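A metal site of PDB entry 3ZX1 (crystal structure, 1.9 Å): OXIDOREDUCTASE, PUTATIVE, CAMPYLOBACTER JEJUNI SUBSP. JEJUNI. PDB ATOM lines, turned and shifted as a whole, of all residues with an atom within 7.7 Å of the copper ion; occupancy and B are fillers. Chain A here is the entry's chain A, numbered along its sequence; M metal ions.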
ATOM      1  N   LEU A 206      27.937  15.214  -2.554  1.00  0.00           N
ATOM      2  CA  LEU A 206      27.595  13.785  -2.654  1.00  0.00           C
ATOM      3  C   LEU A 206      28.697  12.858  -2.054  1.00  0.00           C
ATOM      4  O   LEU A 206      28.396  11.867  -1.369  1.00  0.00           O
ATOM      5  CB  LEU A 206      27.361  13.404  -4.101  1.00  0.00           C
ATOM      6  CG  LEU A 206      26.019  13.890  -4.691  1.00  0.00           C
ATOM      7  CD1 LEU A 206      25.984  13.708  -6.223  1.00  0.00           C
ATOM      8  CD2 LEU A 206      24.856  13.212  -4.006  1.00  0.00           C
ATOM      9  N   ASN A 207      29.947  13.202  -2.339  1.00  0.00           N
ATOM     10  CA  ASN A 207      31.071  12.326  -2.075  1.00  0.00           C
ATOM     11  C   ASN A 207      31.964  12.729  -0.905  1.00  0.00           C
ATOM     12  O   ASN A 207      32.747  11.911  -0.429  1.00  0.00           O
ATOM     13  CB  ASN A 207      31.923  12.154  -3.340  1.00  0.00           C
ATOM     14  CG  ASN A 207      31.160  11.537  -4.462  1.00  0.00           C
ATOM     15  OD1 ASN A 207      30.328  10.619  -4.269  1.00  0.00           O
ATOM     16  ND2 ASN A 207      31.422  12.015  -5.671  1.00  0.00           N
ATOM     17  N   GLY A 208      31.825  13.958  -0.426  1.00  0.00           N
ATOM     18  CA  GLY A 208      32.842  14.554   0.445  1.00  0.00           C
ATOM     19  C   GLY A 208      33.814  15.231  -0.509  1.00  0.00           C
ATOM     20  O   GLY A 208      34.158  14.688  -1.572  1.00  0.00           O
ATOM     21  N   TYR A 242      40.519   9.240   1.233  1.00  0.00           N
ATOM     22  CA  TYR A 242      40.975   7.978   1.751  1.00  0.00           C
ATOM     23  C   TYR A 242      42.429   7.767   1.320  1.00  0.00           C
ATOM     24  O   TYR A 242      42.762   7.887   0.132  1.00  0.00           O
ATOM     25  CB  TYR A 242      40.075   6.856   1.195  1.00  0.00           C
ATOM     26  CG  TYR A 242      38.801   6.714   1.947  1.00  0.00           C
ATOM     27  CD1 TYR A 242      37.896   7.785   2.050  1.00  0.00           C
ATOM     28  CD2 TYR A 242      38.508   5.525   2.598  1.00  0.00           C
ATOM     29  CE1 TYR A 242      36.712   7.663   2.740  1.00  0.00           C
ATOM     30  CE2 TYR A 242      37.321   5.382   3.295  1.00  0.00           C
ATOM     31  CZ  TYR A 242      36.437   6.448   3.362  1.00  0.00           C
ATOM     32  OH  TYR A 242      35.315   6.306   4.099  1.00  0.00           O
ATOM     33  N   ARG A 300      36.078   3.847  -3.344  1.00  0.00           N
ATOM     34  CA  ARG A 300      35.083   3.985  -2.291  1.00  0.00           C
ATOM     35  C   ARG A 300      33.677   4.259  -2.813  1.00  0.00           C
ATOM     36  O   ARG A 300      32.790   4.683  -2.056  1.00  0.00           O
ATOM     37  CB  ARG A 300      35.511   5.044  -1.255  1.00  0.00           C
ATOM     38  CG  ARG A 300      35.634   6.497  -1.747  1.00  0.00           C
ATOM     39  CD  ARG A 300      36.077   7.357  -0.534  1.00  0.00           C
ATOM     40  NE  ARG A 300      36.209   8.797  -0.808  1.00  0.00           N
ATOM     41  CZ  ARG A 300      35.192   9.650  -0.832  1.00  0.00           C
ATOM     42  NH1 ARG A 300      33.944   9.249  -0.616  1.00  0.00           N
ATOM     43  NH2 ARG A 300      35.441  10.939  -1.088  1.00  0.00           N
ATOM     44  N   MET A 347      24.024   2.916   8.953  1.00  0.00           N
ATOM     45  CA  MET A 347      24.261   4.042   8.094  1.00  0.00           C
ATOM     46  C   MET A 347      23.648   3.726   6.722  1.00  0.00           C
ATOM     47  O   MET A 347      23.847   2.643   6.189  1.00  0.00           O
ATOM     48  CB  MET A 347      25.753   4.320   7.986  1.00  0.00           C
ATOM     49  CG  MET A 347      26.440   4.472   9.350  1.00  0.00           C
ATOM     50  SD  MET A 347      28.232   4.675   9.159  1.00  0.00           S
ATOM     51  CE  MET A 347      28.247   6.449   9.098  1.00  0.00           C
ATOM     52  N   SER A 348      22.905   4.662   6.160  1.00  0.00           N
ATOM     53  CA  SER A 348      22.195   4.371   4.898  1.00  0.00           C
ATOM     54  C   SER A 348      22.069   5.652   4.064  1.00  0.00           C
ATOM     55  O   SER A 348      22.419   6.746   4.542  1.00  0.00           O
ATOM     56  CB  SER A 348      20.849   3.681   5.149  1.00  0.00           C
ATOM     57  OG  SER A 348      19.869   4.541   5.742  1.00  0.00           O
ATOM     58  N   GLU A 349      21.627   5.494   2.821  1.00  0.00           N
ATOM     59  CA  GLU A 349      21.331   6.638   1.955  1.00  0.00           C
ATOM     60  C   GLU A 349      19.972   6.452   1.284  1.00  0.00           C
ATOM     61  O   GLU A 349      19.535   5.334   1.044  1.00  0.00           O
ATOM     62  CB  GLU A 349      22.390   6.812   0.876  1.00  0.00           C
ATOM     63  CG  GLU A 349      23.742   7.200   1.441  1.00  0.00           C
ATOM     64  CD  GLU A 349      24.876   6.928   0.465  1.00  0.00           C
ATOM     65  OE1 GLU A 349      24.695   7.121  -0.755  1.00  0.00           O
ATOM     66  OE2 GLU A 349      25.951   6.542   0.923  1.00  0.00           O
ATOM     67  N   PHE A 373      21.425  11.325   3.523  1.00  0.00           N
ATOM     68  CA  PHE A 373      22.437  10.580   4.290  1.00  0.00           C
ATOM     69  C   PHE A 373      21.890  10.371   5.698  1.00  0.00           C
ATOM     70  O   PHE A 373      21.726  11.343   6.451  1.00  0.00           O
ATOM     71  CB  PHE A 373      23.731  11.391   4.282  1.00  0.00           C
ATOM     72  CG  PHE A 373      24.373  11.478   2.929  1.00  0.00           C
ATOM     73  CD1 PHE A 373      25.100  10.405   2.413  1.00  0.00           C
ATOM     74  CD2 PHE A 373      24.267  12.624   2.156  1.00  0.00           C
ATOM     75  CE1 PHE A 373      25.696  10.459   1.145  1.00  0.00           C
ATOM     76  CE2 PHE A 373      24.853  12.698   0.899  1.00  0.00           C
ATOM     77  CZ  PHE A 373      25.554  11.616   0.376  1.00  0.00           C
ATOM     78  N   ASN A 401      26.946  -0.563   7.635  1.00  0.00           N
ATOM     79  CA  ASN A 401      26.824   0.299   6.491  1.00  0.00           C
ATOM     80  C   ASN A 401      25.935  -0.331   5.412  1.00  0.00           C
ATOM     81  O   ASN A 401      26.377  -1.189   4.665  1.00  0.00           O
ATOM     82  CB  ASN A 401      28.213   0.621   5.951  1.00  0.00           C
ATOM     83  CG  ASN A 401      28.194   1.625   4.843  1.00  0.00           C
ATOM     84  OD1 ASN A 401      27.149   2.092   4.425  1.00  0.00           O
ATOM     85  ND2 ASN A 401      29.370   1.951   4.336  1.00  0.00           N
ATOM     86  N   SER A 403      24.721   1.263   2.822  1.00  0.00           N
ATOM     87  CA  SER A 403      24.757   2.043   1.606  1.00  0.00           C
ATOM     88  C   SER A 403      25.823   1.490   0.688  1.00  0.00           C
ATOM     89  O   SER A 403      26.628   0.648   1.090  1.00  0.00           O
ATOM     90  CB  SER A 403      25.084   3.498   1.933  1.00  0.00           C
ATOM     91  OG  SER A 403      26.465   3.608   2.202  1.00  0.00           O
ATOM     92  N   MET A 405      28.445   3.020  -0.472  1.00  0.00           N
ATOM     93  CA  MET A 405      29.738   3.724  -0.404  1.00  0.00           C
ATOM     94  C   MET A 405      30.320   3.734   1.005  1.00  0.00           C
ATOM     95  O   MET A 405      29.572   3.627   1.960  1.00  0.00           O
ATOM     96  CB  MET A 405      29.604   5.162  -0.955  1.00  0.00           C
ATOM     97  CG  MET A 405      29.016   6.153   0.047  1.00  0.00           C
ATOM     98  SD  MET A 405      28.617   7.799  -0.609  1.00  0.00           S
ATOM     99  CE  MET A 405      30.238   8.368  -1.145  1.00  0.00           C
ATOM    100  N   ASP A 406      31.644   3.768   1.140  1.00  0.00           N
ATOM    101  CA  ASP A 406      32.293   3.774   2.463  1.00  0.00           C
ATOM    102  C   ASP A 406      31.849   5.017   3.267  1.00  0.00           C
ATOM    103  O   ASP A 406      31.593   6.100   2.674  1.00  0.00           O
ATOM    104  CB  ASP A 406      33.807   3.767   2.349  1.00  0.00           C
ATOM    105  CG  ASP A 406      34.351   2.571   1.571  1.00  0.00           C
ATOM    106  OD1 ASP A 406      33.929   2.341   0.399  1.00  0.00           O
ATOM    107  OD2 ASP A 406      35.225   1.886   2.138  1.00  0.00           O
ATOM    108  N   HIS A 407      31.711   4.878   4.582  1.00  0.00           N
ATOM    109  CA  HIS A 407      31.560   6.035   5.466  1.00  0.00           C
ATOM    110  C   HIS A 407      32.387   5.779   6.702  1.00  0.00           C
ATOM    111  O   HIS A 407      32.246   4.684   7.336  1.00  0.00           O
ATOM    112  CB  HIS A 407      30.134   6.278   5.920  1.00  0.00           C
ATOM    113  CG  HIS A 407      29.148   6.387   4.810  1.00  0.00           C
ATOM    114  ND1 HIS A 407      28.866   7.589   4.194  1.00  0.00           N
ATOM    115  CD2 HIS A 407      28.343   5.462   4.230  1.00  0.00           C
ATOM    116  CE1 HIS A 407      27.956   7.391   3.261  1.00  0.00           C
ATOM    117  NE2 HIS A 407      27.611   6.106   3.266  1.00  0.00           N
ATOM    118  N   PRO A 408      33.209   6.762   7.082  1.00  0.00           N
ATOM    119  CA  PRO A 408      34.001   6.551   8.309  1.00  0.00           C
ATOM    120  C   PRO A 408      33.200   7.006   9.544  1.00  0.00           C
ATOM    121  O   PRO A 408      32.779   8.154   9.606  1.00  0.00           O
ATOM    122  CB  PRO A 408      35.272   7.397   8.080  1.00  0.00           C
ATOM    123  CG  PRO A 408      34.814   8.586   7.161  1.00  0.00           C
ATOM    124  CD  PRO A 408      33.546   8.038   6.394  1.00  0.00           C
ATOM    125  N   PHE A 409      32.982   6.104  10.497  1.00  0.00           N
ATOM    126  CA  PHE A 409      32.156   6.377  11.664  1.00  0.00           C
ATOM    127  C   PHE A 409      32.969   7.000  12.794  1.00  0.00           C
ATOM    128  O   PHE A 409      34.039   6.495  13.122  1.00  0.00           O
ATOM    129  CB  PHE A 409      31.572   5.056  12.193  1.00  0.00           C
ATOM    130  CG  PHE A 409      30.890   5.181  13.538  1.00  0.00           C
ATOM    131  CD1 PHE A 409      29.561   5.649  13.622  1.00  0.00           C
ATOM    132  CD2 PHE A 409      31.547   4.811  14.722  1.00  0.00           C
ATOM    133  CE1 PHE A 409      28.884   5.735  14.869  1.00  0.00           C
ATOM    134  CE2 PHE A 409      30.910   4.932  15.974  1.00  0.00           C
ATOM    135  CZ  PHE A 409      29.556   5.391  16.050  1.00  0.00           C
ATOM    136  N   HIS A 462      28.714  10.283  14.141  1.00  0.00           N
ATOM    137  CA  HIS A 462      28.369  10.699  12.773  1.00  0.00           C
ATOM    138  C   HIS A 462      29.333  10.120  11.809  1.00  0.00           C
ATOM    139  O   HIS A 462      30.358   9.555  12.198  1.00  0.00           O
ATOM    140  CB  HIS A 462      28.377  12.244  12.636  1.00  0.00           C
ATOM    141  CG  HIS A 462      29.613  12.893  13.211  1.00  0.00           C
ATOM    142  ND1 HIS A 462      30.674  13.302  12.424  1.00  0.00           N
ATOM    143  CD2 HIS A 462      29.939  13.207  14.481  1.00  0.00           C
ATOM    144  CE1 HIS A 462      31.601  13.858  13.201  1.00  0.00           C
ATOM    145  NE2 HIS A 462      31.190  13.805  14.445  1.00  0.00           N
ATOM    146  N   CYS A 463      28.970  10.205  10.540  1.00  0.00           N
ATOM    147  CA  CYS A 463      29.920   9.964   9.472  1.00  0.00           C
ATOM    148  C   CYS A 463      30.932  11.095   9.517  1.00  0.00           C
ATOM    149  O   CYS A 463      30.553  12.232   9.788  1.00  0.00           O
ATOM    150  CB  CYS A 463      29.227  10.003   8.112  1.00  0.00           C
ATOM    151  SG  CYS A 463      30.429   9.864   6.836  1.00  0.00           S
ATOM    152  N   HIS A 464      32.192  10.793   9.292  1.00  0.00           N
ATOM    153  CA  HIS A 464      33.198  11.837   9.356  1.00  0.00           C
ATOM    154  C   HIS A 464      33.633  12.303   7.950  1.00  0.00           C
ATOM    155  O   HIS A 464      34.647  13.011   7.825  1.00  0.00           O
ATOM    156  CB  HIS A 464      34.406  11.485  10.264  1.00  0.00           C
ATOM    157  CG  HIS A 464      34.983  12.691  10.947  1.00  0.00           C
ATOM    158  ND1 HIS A 464      35.688  13.659  10.262  1.00  0.00           N
ATOM    159  CD2 HIS A 464      34.880  13.138  12.223  1.00  0.00           C
ATOM    160  CE1 HIS A 464      36.025  14.629  11.084  1.00  0.00           C
ATOM    161  NE2 HIS A 464      35.555  14.335  12.281  1.00  0.00           N
ATOM    162  N   ILE A 465      32.885  11.922   6.916  1.00  0.00           N
ATOM    163  CA  ILE A 465      32.990  12.654   5.655  1.00  0.00           C
ATOM    164  C   ILE A 465      32.219  13.949   5.937  1.00  0.00           C
ATOM    165  O   ILE A 465      31.001  13.927   6.133  1.00  0.00           O
ATOM    166  CB  ILE A 465      32.432  11.864   4.435  1.00  0.00           C
ATOM    167  CG1 ILE A 465      33.424  10.747   4.018  1.00  0.00           C
ATOM    168  CG2 ILE A 465      32.159  12.837   3.252  1.00  0.00           C
ATOM    169  CD1 ILE A 465      32.785   9.599   3.215  1.00  0.00           C
ATOM    170  N   LEU A 466      32.941  15.062   6.014  1.00  0.00           N
ATOM    171  CA  LEU A 466      32.384  16.277   6.605  1.00  0.00           C
ATOM    172  C   LEU A 466      31.138  16.734   5.883  1.00  0.00           C
ATOM    173  O   LEU A 466      30.188  17.170   6.527  1.00  0.00           O
ATOM    174  CB  LEU A 466      33.422  17.414   6.636  1.00  0.00           C
ATOM    175  CG  LEU A 466      34.640  17.173   7.539  1.00  0.00           C
ATOM    176  CD1 LEU A 466      35.474  18.424   7.575  1.00  0.00           C
ATOM    177  CD2 LEU A 466      34.294  16.821   8.962  1.00  0.00           C
ATOM    178  N   GLU A 467      31.094  16.595   4.563  1.00  0.00           N
ATOM    179  CA  GLU A 467      29.912  17.039   3.851  1.00  0.00           C
ATOM    180  C   GLU A 467      28.682  16.201   4.245  1.00  0.00           C
ATOM    181  O   GLU A 467      27.577  16.747   4.350  1.00  0.00           O
ATOM    182  CB  GLU A 467      30.100  17.029   2.337  1.00  0.00           C
ATOM    183  CG  GLU A 467      30.956  18.153   1.749  1.00  0.00           C
ATOM    184  CD  GLU A 467      32.414  18.130   2.174  1.00  0.00           C
ATOM    185  OE1 GLU A 467      32.948  17.054   2.583  1.00  0.00           O
ATOM    186  OE2 GLU A 467      33.027  19.221   2.118  1.00  0.00           O
ATOM    187  N   HIS A 468      28.871  14.891   4.492  1.00  0.00           N
ATOM    188  CA  HIS A 468      27.747  14.019   4.935  1.00  0.00           C
ATOM    189  C   HIS A 468      27.253  14.399   6.320  1.00  0.00           C
ATOM    190  O   HIS A 468      26.031  14.480   6.567  1.00  0.00           O
ATOM    191  CB  HIS A 468      28.159  12.533   4.954  1.00  0.00           C
ATOM    192  CG  HIS A 468      28.478  12.003   3.596  1.00  0.00           C
ATOM    193  ND1 HIS A 468      28.920  10.718   3.388  1.00  0.00           N
ATOM    194  CD2 HIS A 468      28.407  12.587   2.364  1.00  0.00           C
ATOM    195  CE1 HIS A 468      29.120  10.527   2.089  1.00  0.00           C
ATOM    196  NE2 HIS A 468      28.807  11.639   1.448  1.00  0.00           N
ATOM    197  N   GLU A 469      28.206  14.672   7.208  1.00  0.00           N
ATOM    198  CA  GLU A 469      27.888  15.174   8.542  1.00  0.00           C
ATOM    199  C   GLU A 469      27.025  16.431   8.451  1.00  0.00           C
ATOM    200  O   GLU A 469      25.973  16.480   9.074  1.00  0.00           O
ATOM    201  CB  GLU A 469      29.171  15.388   9.354  1.00  0.00           C
ATOM    202  CG  GLU A 469      29.166  16.467  10.413  1.00  0.00           C
ATOM    203  CD  GLU A 469      30.603  16.832  10.826  1.00  0.00           C
ATOM    204  OE1 GLU A 469      31.448  15.927  10.911  1.00  0.00           O
ATOM    205  OE2 GLU A 469      30.893  18.024  11.032  1.00  0.00           O
ATOM    206  N   MET A 473      24.104  13.432   8.560  1.00  0.00           N
ATOM    207  CA  MET A 473      24.417  12.025   8.818  1.00  0.00           C
ATOM    208  C   MET A 473      25.033  11.903  10.188  1.00  0.00           C
ATOM    209  O   MET A 473      26.227  11.616  10.322  1.00  0.00           O
ATOM    210  CB  MET A 473      25.342  11.455   7.740  1.00  0.00           C
ATOM    211  CG  MET A 473      25.390   9.893   7.734  1.00  0.00           C
ATOM    212  SD  MET A 473      26.272   9.222   6.295  1.00  0.00           S
ATOM    213  CE  MET A 473      25.665   7.547   6.327  1.00  0.00           C
HETATM  214 CU    CU M   1      29.317   9.437   4.873  1.00  0.00          CU
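Merely in contact with the copper ion: Met 473 (3.4 Å) and Ile 465 (3.8 Å). Of the 25 residues printed, 5 come within 4 Å of the copper ion.
The copper ion is bound by a ring nitrogen (ND1) of His 468 (2.0 Å), a ring nitrogen (ND1) of His 407 (2.0 Å) and the side-chain sulfur (SG) of Cys 463 (2.3 Å). The copper ion has three donor atoms within binding distance.
The backbone carbonyl oxygen of His 468 lies within hydrogen-bond range of the backbone NH of Met 473, 3.0 Å away. NE2 of His 468 sits at hydrogen-bond distance from O of Leu 206, 2.9 Å away. A ring nitrogen (ND1) of His 407 sits close to the side-chain sulfur (SD) of Met 473 (3.7 Å). NE2 of His 407 sits close to O of Met 405, 3.4 Å away. A ring nitrogen (NE2) of His 407 is in hydrogen-bond range of the side-chain carboxylate (OE2) of Glu 349 (2.9 Å). OG of Ser 403 lies within hydrogen-bond range of NE2 of His 407 (2.9 Å). The backbone carbonyl oxygen (O) of Met 473 is in hydrogen-bond range of the backbone NH (N) of Cys 463, 3.1 Å away. N of Ile 465 lies close to SG of Cys 463 (3.2 Å).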
